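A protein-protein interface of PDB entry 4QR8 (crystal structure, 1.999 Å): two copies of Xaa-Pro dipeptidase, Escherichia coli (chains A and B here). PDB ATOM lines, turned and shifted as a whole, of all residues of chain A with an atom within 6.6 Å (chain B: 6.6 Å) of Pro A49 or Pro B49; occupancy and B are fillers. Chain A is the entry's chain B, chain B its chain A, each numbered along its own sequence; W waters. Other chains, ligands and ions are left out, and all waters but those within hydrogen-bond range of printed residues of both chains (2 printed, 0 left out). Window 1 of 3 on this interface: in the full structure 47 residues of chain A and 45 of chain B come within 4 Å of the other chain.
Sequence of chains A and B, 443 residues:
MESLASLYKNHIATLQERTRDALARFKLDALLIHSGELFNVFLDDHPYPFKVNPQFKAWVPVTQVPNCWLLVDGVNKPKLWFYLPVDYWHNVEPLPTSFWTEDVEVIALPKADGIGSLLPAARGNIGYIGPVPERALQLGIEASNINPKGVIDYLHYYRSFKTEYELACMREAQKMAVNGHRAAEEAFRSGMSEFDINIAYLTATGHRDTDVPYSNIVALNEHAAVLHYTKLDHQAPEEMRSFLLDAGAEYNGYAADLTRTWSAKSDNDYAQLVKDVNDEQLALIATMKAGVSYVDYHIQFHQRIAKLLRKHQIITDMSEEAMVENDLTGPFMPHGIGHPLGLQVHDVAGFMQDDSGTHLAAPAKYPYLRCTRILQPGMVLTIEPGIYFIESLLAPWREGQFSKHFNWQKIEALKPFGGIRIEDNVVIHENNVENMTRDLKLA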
ATOM      1  N   LEU A  38      12.600 -27.399  -8.663  1.00  0.00           N
ATOM      2  CA  LEU A  38      11.862 -26.149  -8.657  1.00  0.00           C
ATOM      3  C   LEU A  38      12.658 -25.081  -9.390  1.00  0.00           C
ATOM      4  O   LEU A  38      13.885 -25.064  -9.334  1.00  0.00           O
ATOM      5  CB  LEU A  38      11.591 -25.701  -7.222  1.00  0.00           C
ATOM      6  CG  LEU A  38      10.721 -26.663  -6.415  1.00  0.00           C
ATOM      7  CD1 LEU A  38      10.519 -26.147  -4.999  1.00  0.00           C
ATOM      8  CD2 LEU A  38       9.389 -26.858  -7.122  1.00  0.00           C
ATOM      9  N   PHE A  39      11.955 -24.200 -10.091  1.00  0.00           N
ATOM     10  CA  PHE A  39      12.580 -23.019 -10.678  1.00  0.00           C
ATOM     11  C   PHE A  39      11.649 -21.820 -10.534  1.00  0.00           C
ATOM     12  O   PHE A  39      10.424 -21.967 -10.557  1.00  0.00           O
ATOM     13  CB  PHE A  39      12.964 -23.255 -12.140  1.00  0.00           C
ATOM     14  CG  PHE A  39      11.833 -23.735 -13.000  1.00  0.00           C
ATOM     15  CD1 PHE A  39      11.070 -22.839 -13.728  1.00  0.00           C
ATOM     16  CD2 PHE A  39      11.539 -25.086 -13.090  1.00  0.00           C
ATOM     17  CE1 PHE A  39      10.029 -23.280 -14.526  1.00  0.00           C
ATOM     18  CE2 PHE A  39      10.500 -25.532 -13.883  1.00  0.00           C
ATOM     19  CZ  PHE A  39       9.744 -24.627 -14.602  1.00  0.00           C
ATOM     20  N   HIS A  46       9.396 -16.383  -6.629  1.00  0.00           N
ATOM     21  CA  HIS A  46       8.115 -17.066  -6.796  1.00  0.00           C
ATOM     22  C   HIS A  46       8.322 -18.300  -7.673  1.00  0.00           C
ATOM     23  O   HIS A  46       8.712 -18.183  -8.834  1.00  0.00           O
ATOM     24  CB  HIS A  46       7.106 -16.106  -7.444  1.00  0.00           C
ATOM     25  CG  HIS A  46       5.735 -16.683  -7.636  1.00  0.00           C
ATOM     26  ND1 HIS A  46       4.769 -16.053  -8.391  1.00  0.00           N
ATOM     27  CD2 HIS A  46       5.168 -17.822  -7.171  1.00  0.00           C
ATOM     28  CE1 HIS A  46       3.666 -16.780  -8.386  1.00  0.00           C
ATOM     29  NE2 HIS A  46       3.881 -17.857  -7.654  1.00  0.00           N
ATOM     30  N   PRO A  47       8.076 -19.494  -7.115  1.00  0.00           N
ATOM     31  CA  PRO A  47       8.306 -20.730  -7.868  1.00  0.00           C
ATOM     32  C   PRO A  47       7.155 -21.064  -8.809  1.00  0.00           C
ATOM     33  O   PRO A  47       5.995 -20.838  -8.469  1.00  0.00           O
ATOM     34  CB  PRO A  47       8.392 -21.801  -6.771  1.00  0.00           C
ATOM     35  CG  PRO A  47       8.408 -21.055  -5.461  1.00  0.00           C
ATOM     36  CD  PRO A  47       7.700 -19.768  -5.723  1.00  0.00           C
ATOM     37  N   TYR A  48       7.478 -21.594  -9.985  1.00  0.00           N
ATOM     38  CA  TYR A  48       6.462 -22.172 -10.853  1.00  0.00           C
ATOM     39  C   TYR A  48       5.934 -23.416 -10.145  1.00  0.00           C
ATOM     40  O   TYR A  48       6.630 -23.987  -9.304  1.00  0.00           O
ATOM     41  CB  TYR A  48       7.067 -22.552 -12.209  1.00  0.00           C
ATOM     42  CG  TYR A  48       7.270 -21.386 -13.157  1.00  0.00           C
ATOM     43  CD1 TYR A  48       8.437 -20.628 -13.126  1.00  0.00           C
ATOM     44  CD2 TYR A  48       6.299 -21.051 -14.096  1.00  0.00           C
ATOM     45  CE1 TYR A  48       8.627 -19.572 -13.996  1.00  0.00           C
ATOM     46  CE2 TYR A  48       6.483 -19.991 -14.970  1.00  0.00           C
ATOM     47  CZ  TYR A  48       7.648 -19.255 -14.914  1.00  0.00           C
ATOM     48  OH  TYR A  48       7.836 -18.201 -15.780  1.00  0.00           O
ATOM     49  N   PRO A  49       4.700 -23.836 -10.460  1.00  0.00           N
ATOM     50  CA  PRO A  49       4.214 -25.080  -9.853  1.00  0.00           C
ATOM     51  C   PRO A  49       5.113 -26.248 -10.242  1.00  0.00           C
ATOM     52  O   PRO A  49       5.624 -26.276 -11.365  1.00  0.00           O
ATOM     53  CB  PRO A  49       2.819 -25.253 -10.466  1.00  0.00           C
ATOM     54  CG  PRO A  49       2.835 -24.416 -11.710  1.00  0.00           C
ATOM     55  CD  PRO A  49       3.714 -23.249 -11.382  1.00  0.00           C
ATOM     56  N   PHE A  50       5.326 -27.185  -9.325  1.00  0.00           N
ATOM     57  CA  PHE A  50       6.160 -28.340  -9.633  1.00  0.00           C
ATOM     58  C   PHE A  50       5.423 -29.330 -10.526  1.00  0.00           C
ATOM     59  O   PHE A  50       4.322 -29.781 -10.198  1.00  0.00           O
ATOM     60  CB  PHE A  50       6.649 -29.038  -8.363  1.00  0.00           C
ATOM     61  CG  PHE A  50       7.490 -30.257  -8.634  1.00  0.00           C
ATOM     62  CD1 PHE A  50       8.716 -30.138  -9.270  1.00  0.00           C
ATOM     63  CD2 PHE A  50       7.052 -31.519  -8.262  1.00  0.00           C
ATOM     64  CE1 PHE A  50       9.488 -31.258  -9.528  1.00  0.00           C
ATOM     65  CE2 PHE A  50       7.819 -32.638  -8.515  1.00  0.00           C
ATOM     66  CZ  PHE A  50       9.037 -32.510  -9.145  1.00  0.00           C
ATOM     67  N   LYS A  51       6.037 -29.658 -11.658  1.00  0.00           N
ATOM     68  CA  LYS A  51       5.504 -30.671 -12.564  1.00  0.00           C
ATOM     69  C   LYS A  51       6.513 -31.802 -12.706  1.00  0.00           C
ATOM     70  O   LYS A  51       7.532 -31.650 -13.381  1.00  0.00           O
ATOM     71  CB  LYS A  51       5.204 -30.069 -13.939  1.00  0.00           C
ATOM     72  CG  LYS A  51       4.271 -28.867 -13.910  1.00  0.00           C
ATOM     73  CD  LYS A  51       2.887 -29.231 -13.395  1.00  0.00           C
ATOM     74  CE  LYS A  51       1.986 -28.003 -13.343  1.00  0.00           C
ATOM     75  NZ  LYS A  51       0.615 -28.324 -12.862  1.00  0.00           N
ATOM     76  N   THR A 210      -4.196 -25.657  -9.893  1.00  0.00           N
ATOM     77  CA  THR A 210      -2.759 -25.857 -10.022  1.00  0.00           C
ATOM     78  C   THR A 210      -2.366 -27.329 -10.132  1.00  0.00           C
ATOM     79  O   THR A 210      -1.211 -27.637 -10.418  1.00  0.00           O
ATOM     80  CB  THR A 210      -1.990 -25.229  -8.837  1.00  0.00           C
ATOM     81  OG1 THR A 210      -2.583 -25.652  -7.602  1.00  0.00           O
ATOM     82  CG2 THR A 210      -2.029 -23.709  -8.915  1.00  0.00           C
ATOM     83  N   LEU B  38       5.813 -18.798 -23.380  1.00  0.00           N
ATOM     84  CA  LEU B  38       5.316 -20.050 -22.830  1.00  0.00           C
ATOM     85  C   LEU B  38       6.393 -21.116 -22.963  1.00  0.00           C
ATOM     86  O   LEU B  38       7.226 -21.059 -23.869  1.00  0.00           O
ATOM     87  CB  LEU B  38       4.056 -20.496 -23.574  1.00  0.00           C
ATOM     88  CG  LEU B  38       2.689 -19.983 -23.116  1.00  0.00           C
ATOM     89  CD1 LEU B  38       2.806 -18.747 -22.234  1.00  0.00           C
ATOM     90  CD2 LEU B  38       1.815 -19.693 -24.329  1.00  0.00           C
ATOM     91  N   PHE B  39       6.386 -22.077 -22.047  1.00  0.00           N
ATOM     92  CA  PHE B  39       7.248 -23.248 -22.161  1.00  0.00           C
ATOM     93  C   PHE B  39       6.577 -24.465 -21.527  1.00  0.00           C
ATOM     94  O   PHE B  39       5.784 -24.330 -20.594  1.00  0.00           O
ATOM     95  CB  PHE B  39       8.637 -22.988 -21.561  1.00  0.00           C
ATOM     96  CG  PHE B  39       8.609 -22.370 -20.192  1.00  0.00           C
ATOM     97  CD1 PHE B  39       8.529 -23.164 -19.059  1.00  0.00           C
ATOM     98  CD2 PHE B  39       8.683 -20.994 -20.037  1.00  0.00           C
ATOM     99  CE1 PHE B  39       8.510 -22.598 -17.797  1.00  0.00           C
ATOM    100  CE2 PHE B  39       8.664 -20.421 -18.778  1.00  0.00           C
ATOM    101  CZ  PHE B  39       8.578 -21.224 -17.657  1.00  0.00           C
ATOM    102  N   HIS B  46       2.188 -30.007 -22.073  1.00  0.00           N
ATOM    103  CA  HIS B  46       1.493 -29.288 -21.015  1.00  0.00           C
ATOM    104  C   HIS B  46       2.292 -28.041 -20.653  1.00  0.00           C
ATOM    105  O   HIS B  46       3.421 -28.138 -20.178  1.00  0.00           O
ATOM    106  CB  HIS B  46       1.341 -30.197 -19.792  1.00  0.00           C
ATOM    107  CG  HIS B  46       0.566 -29.586 -18.666  1.00  0.00           C
ATOM    108  ND1 HIS B  46       0.572 -30.111 -17.392  1.00  0.00           N
ATOM    109  CD2 HIS B  46      -0.245 -28.502 -18.623  1.00  0.00           C
ATOM    110  CE1 HIS B  46      -0.198 -29.374 -16.610  1.00  0.00           C
ATOM    111  NE2 HIS B  46      -0.705 -28.391 -17.333  1.00  0.00           N
ATOM    112  N   PRO B  47       1.713 -26.858 -20.892  1.00  0.00           N
ATOM    113  CA  PRO B  47       2.445 -25.616 -20.639  1.00  0.00           C
ATOM    114  C   PRO B  47       2.446 -25.227 -19.165  1.00  0.00           C
ATOM    115  O   PRO B  47       1.438 -25.402 -18.479  1.00  0.00           O
ATOM    116  CB  PRO B  47       1.658 -24.573 -21.450  1.00  0.00           C
ATOM    117  CG  PRO B  47       0.736 -25.363 -22.343  1.00  0.00           C
ATOM    118  CD  PRO B  47       0.437 -26.606 -21.575  1.00  0.00           C
ATOM    119  N   TYR B  48       3.575 -24.717 -18.686  1.00  0.00           N
ATOM    120  CA  TYR B  48       3.614 -24.073 -17.383  1.00  0.00           C
ATOM    121  C   TYR B  48       2.749 -22.827 -17.479  1.00  0.00           C
ATOM    122  O   TYR B  48       2.610 -22.254 -18.557  1.00  0.00           O
ATOM    123  CB  TYR B  48       5.048 -23.684 -17.011  1.00  0.00           C
ATOM    124  CG  TYR B  48       5.896 -24.834 -16.518  1.00  0.00           C
ATOM    125  CD1 TYR B  48       6.633 -25.609 -17.402  1.00  0.00           C
ATOM    126  CD2 TYR B  48       5.963 -25.140 -15.163  1.00  0.00           C
ATOM    127  CE1 TYR B  48       7.411 -26.663 -16.953  1.00  0.00           C
ATOM    128  CE2 TYR B  48       6.738 -26.191 -14.705  1.00  0.00           C
ATOM    129  CZ  TYR B  48       7.461 -26.949 -15.603  1.00  0.00           C
ATOM    130  OH  TYR B  48       8.236 -27.996 -15.151  1.00  0.00           O
ATOM    131  N   PRO B  49       2.147 -22.409 -16.358  1.00  0.00           N
ATOM    132  CA  PRO B  49       1.361 -21.174 -16.386  1.00  0.00           C
ATOM    133  C   PRO B  49       2.253 -19.982 -16.711  1.00  0.00           C
ATOM    134  O   PRO B  49       3.412 -19.946 -16.293  1.00  0.00           O
ATOM    135  CB  PRO B  49       0.822 -21.070 -14.958  1.00  0.00           C
ATOM    136  CG  PRO B  49       1.764 -21.892 -14.134  1.00  0.00           C
ATOM    137  CD  PRO B  49       2.188 -23.016 -15.018  1.00  0.00           C
ATOM    138  N   PHE B  50       1.727 -19.023 -17.466  1.00  0.00           N
ATOM    139  CA  PHE B  50       2.510 -17.854 -17.832  1.00  0.00           C
ATOM    140  C   PHE B  50       2.654 -16.899 -16.656  1.00  0.00           C
ATOM    141  O   PHE B  50       1.664 -16.456 -16.069  1.00  0.00           O
ATOM    142  CB  PHE B  50       1.896 -17.134 -19.038  1.00  0.00           C
ATOM    143  CG  PHE B  50       2.609 -15.859 -19.409  1.00  0.00           C
ATOM    144  CD1 PHE B  50       3.896 -15.893 -19.922  1.00  0.00           C
ATOM    145  CD2 PHE B  50       1.989 -14.630 -19.254  1.00  0.00           C
ATOM    146  CE1 PHE B  50       4.555 -14.729 -20.265  1.00  0.00           C
ATOM    147  CE2 PHE B  50       2.644 -13.460 -19.594  1.00  0.00           C
ATOM    148  CZ  PHE B  50       3.931 -13.508 -20.100  1.00  0.00           C
ATOM    149  N   LYS B  51       3.901 -16.597 -16.314  1.00  0.00           N
ATOM    150  CA  LYS B  51       4.215 -15.630 -15.273  1.00  0.00           C
ATOM    151  C   LYS B  51       5.000 -14.480 -15.890  1.00  0.00           C
ATOM    152  O   LYS B  51       6.166 -14.633 -16.261  1.00  0.00           O
ATOM    153  CB  LYS B  51       5.025 -16.286 -14.157  1.00  0.00           C
ATOM    154  CG  LYS B  51       4.339 -17.482 -13.512  1.00  0.00           C
ATOM    155  CD  LYS B  51       3.044 -17.072 -12.824  1.00  0.00           C
ATOM    156  CE  LYS B  51       2.354 -18.269 -12.196  1.00  0.00           C
ATOM    157  NZ  LYS B  51       1.123 -17.859 -11.467  1.00  0.00           N
ATOM    158  N   THR B 210      -4.096 -20.389  -9.668  1.00  0.00           N
ATOM    159  CA  THR B 210      -3.078 -20.152 -10.683  1.00  0.00           C
ATOM    160  C   THR B 210      -2.764 -18.672 -10.923  1.00  0.00           C
ATOM    161  O   THR B 210      -1.830 -18.357 -11.657  1.00  0.00           O
ATOM    162  CB  THR B 210      -3.475 -20.788 -12.034  1.00  0.00           C
ATOM    163  OG1 THR B 210      -4.832 -20.451 -12.339  1.00  0.00           O
ATOM    164  CG2 THR B 210      -3.341 -22.298 -11.977  1.00  0.00           C
HETATM  165  O   HOH W   1       6.055 -17.639 -17.742  1.00  0.00           O
HETATM  166  O   HOH W   2       8.440 -28.473 -12.397  1.00  0.00           O
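Among the printed residues, pairs that only touch across the chains: Phe A39 with Phe B39 (3.7 Å), Phe A39 with Tyr B48 (3.4 Å), Tyr A48 with Phe B39 (3.5 Å), Tyr A48 with Pro B49 (3.3 Å), Tyr A48 with Lys B51 (3.6 Å), Pro A49 with Tyr B48 (3.5 Å), Pro A49 with Pro B49 (3.6 Å), Lys A51 with His B46 (3.98 Å), Lys A51 with Tyr B48 (3.7 Å) and Thr A210 with Thr B210 (3.6 Å).
Of chain A, only Tyr A48 and Pro A49 come within 4 Å of Pro B49.
Printed residues of chain A within 4 Å of Tyr B48: Phe A39, Pro A49 and Lys A51.
Printed residues of chain A within 4 Å of Thr B210: Thr A210.
Of the printed residues of chain A, Phe B39 touches Phe A39 (3.7 Å) and Tyr A48 (3.5 Å).
Of the printed residues of chain B, Phe A39 touches Phe B39 (3.7 Å) and Tyr B48 (3.4 Å).
Leu A38 touches none of the printed residues of chain B.
The nearest residue of chain B that does not touch Pro A49 is Lys B51 (5.2 Å).
The nearest residue of chain A that does not touch Pro B49 is Lys A51 (5.3 Å).
The nearest printed residue of chain A that does not touch His B46 is Thr A210 (6.5 Å).
Of the 9 printed residues of chain A, 5 touch a printed residue of chain B.
Hydrophobic or aromatic side chains of chain A that line the printed part of chain B: Phe A39, Tyr A48 and Pro A49.
Printed residues of chain B that touch a printed residue of chain A: Phe B39, His B46, Tyr B48, Pro B49, Lys B51 and Thr B210.
Hydrophobic or aromatic side chains of chain B that line the printed part of chain A: Phe B39, His B46, Tyr B48 and Pro B49.
Among the printed residues, 10 pairs touch across the chains.
The backbone carbonyl oxygen (O) of Phe B39 sits at hydrogen-bond distance from the backbone NH (N) of Tyr B48, 2.9 Å away.
NZ of Lys B51 sits at hydrogen-bond distance from O of Thr B210.
O of Phe A39 sits at hydrogen-bond distance from N of Tyr A48, at 3.0 Å.
The side-chain amino group (NZ) of Lys A51 sits at hydrogen-bond distance from the backbone carbonyl oxygen (O) of Thr A210 (3.1 Å).
Water W1 bridges the side-chain hydroxyl (OH) of Tyr A48 (2.7 Å) and the backbone NH (N) of Lys B51 (2.8 Å).
Water W2 lies within hydrogen-bond range of the backbone NH of Lys A51 and the side-chain hydroxyl of Tyr B48.
Phe A39 touches its own counterpart, Phe B39.
Phe A39 touches Tyr B48, and with the chains exchanged Tyr A48 touches Phe B39.
Tyr A48 touches Lys B51, and with the chains exchanged Lys A51 touches Tyr B48.
Thr A210 touches its own counterpart, Thr B210.
Positions printed for both chains: 38, 39, 46, 47, 48, 49, 50, 51 and 210.
Of the 10 pairs that touch across the chains among the printed residues, 9 have their exchanged pair printed and touching as well.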
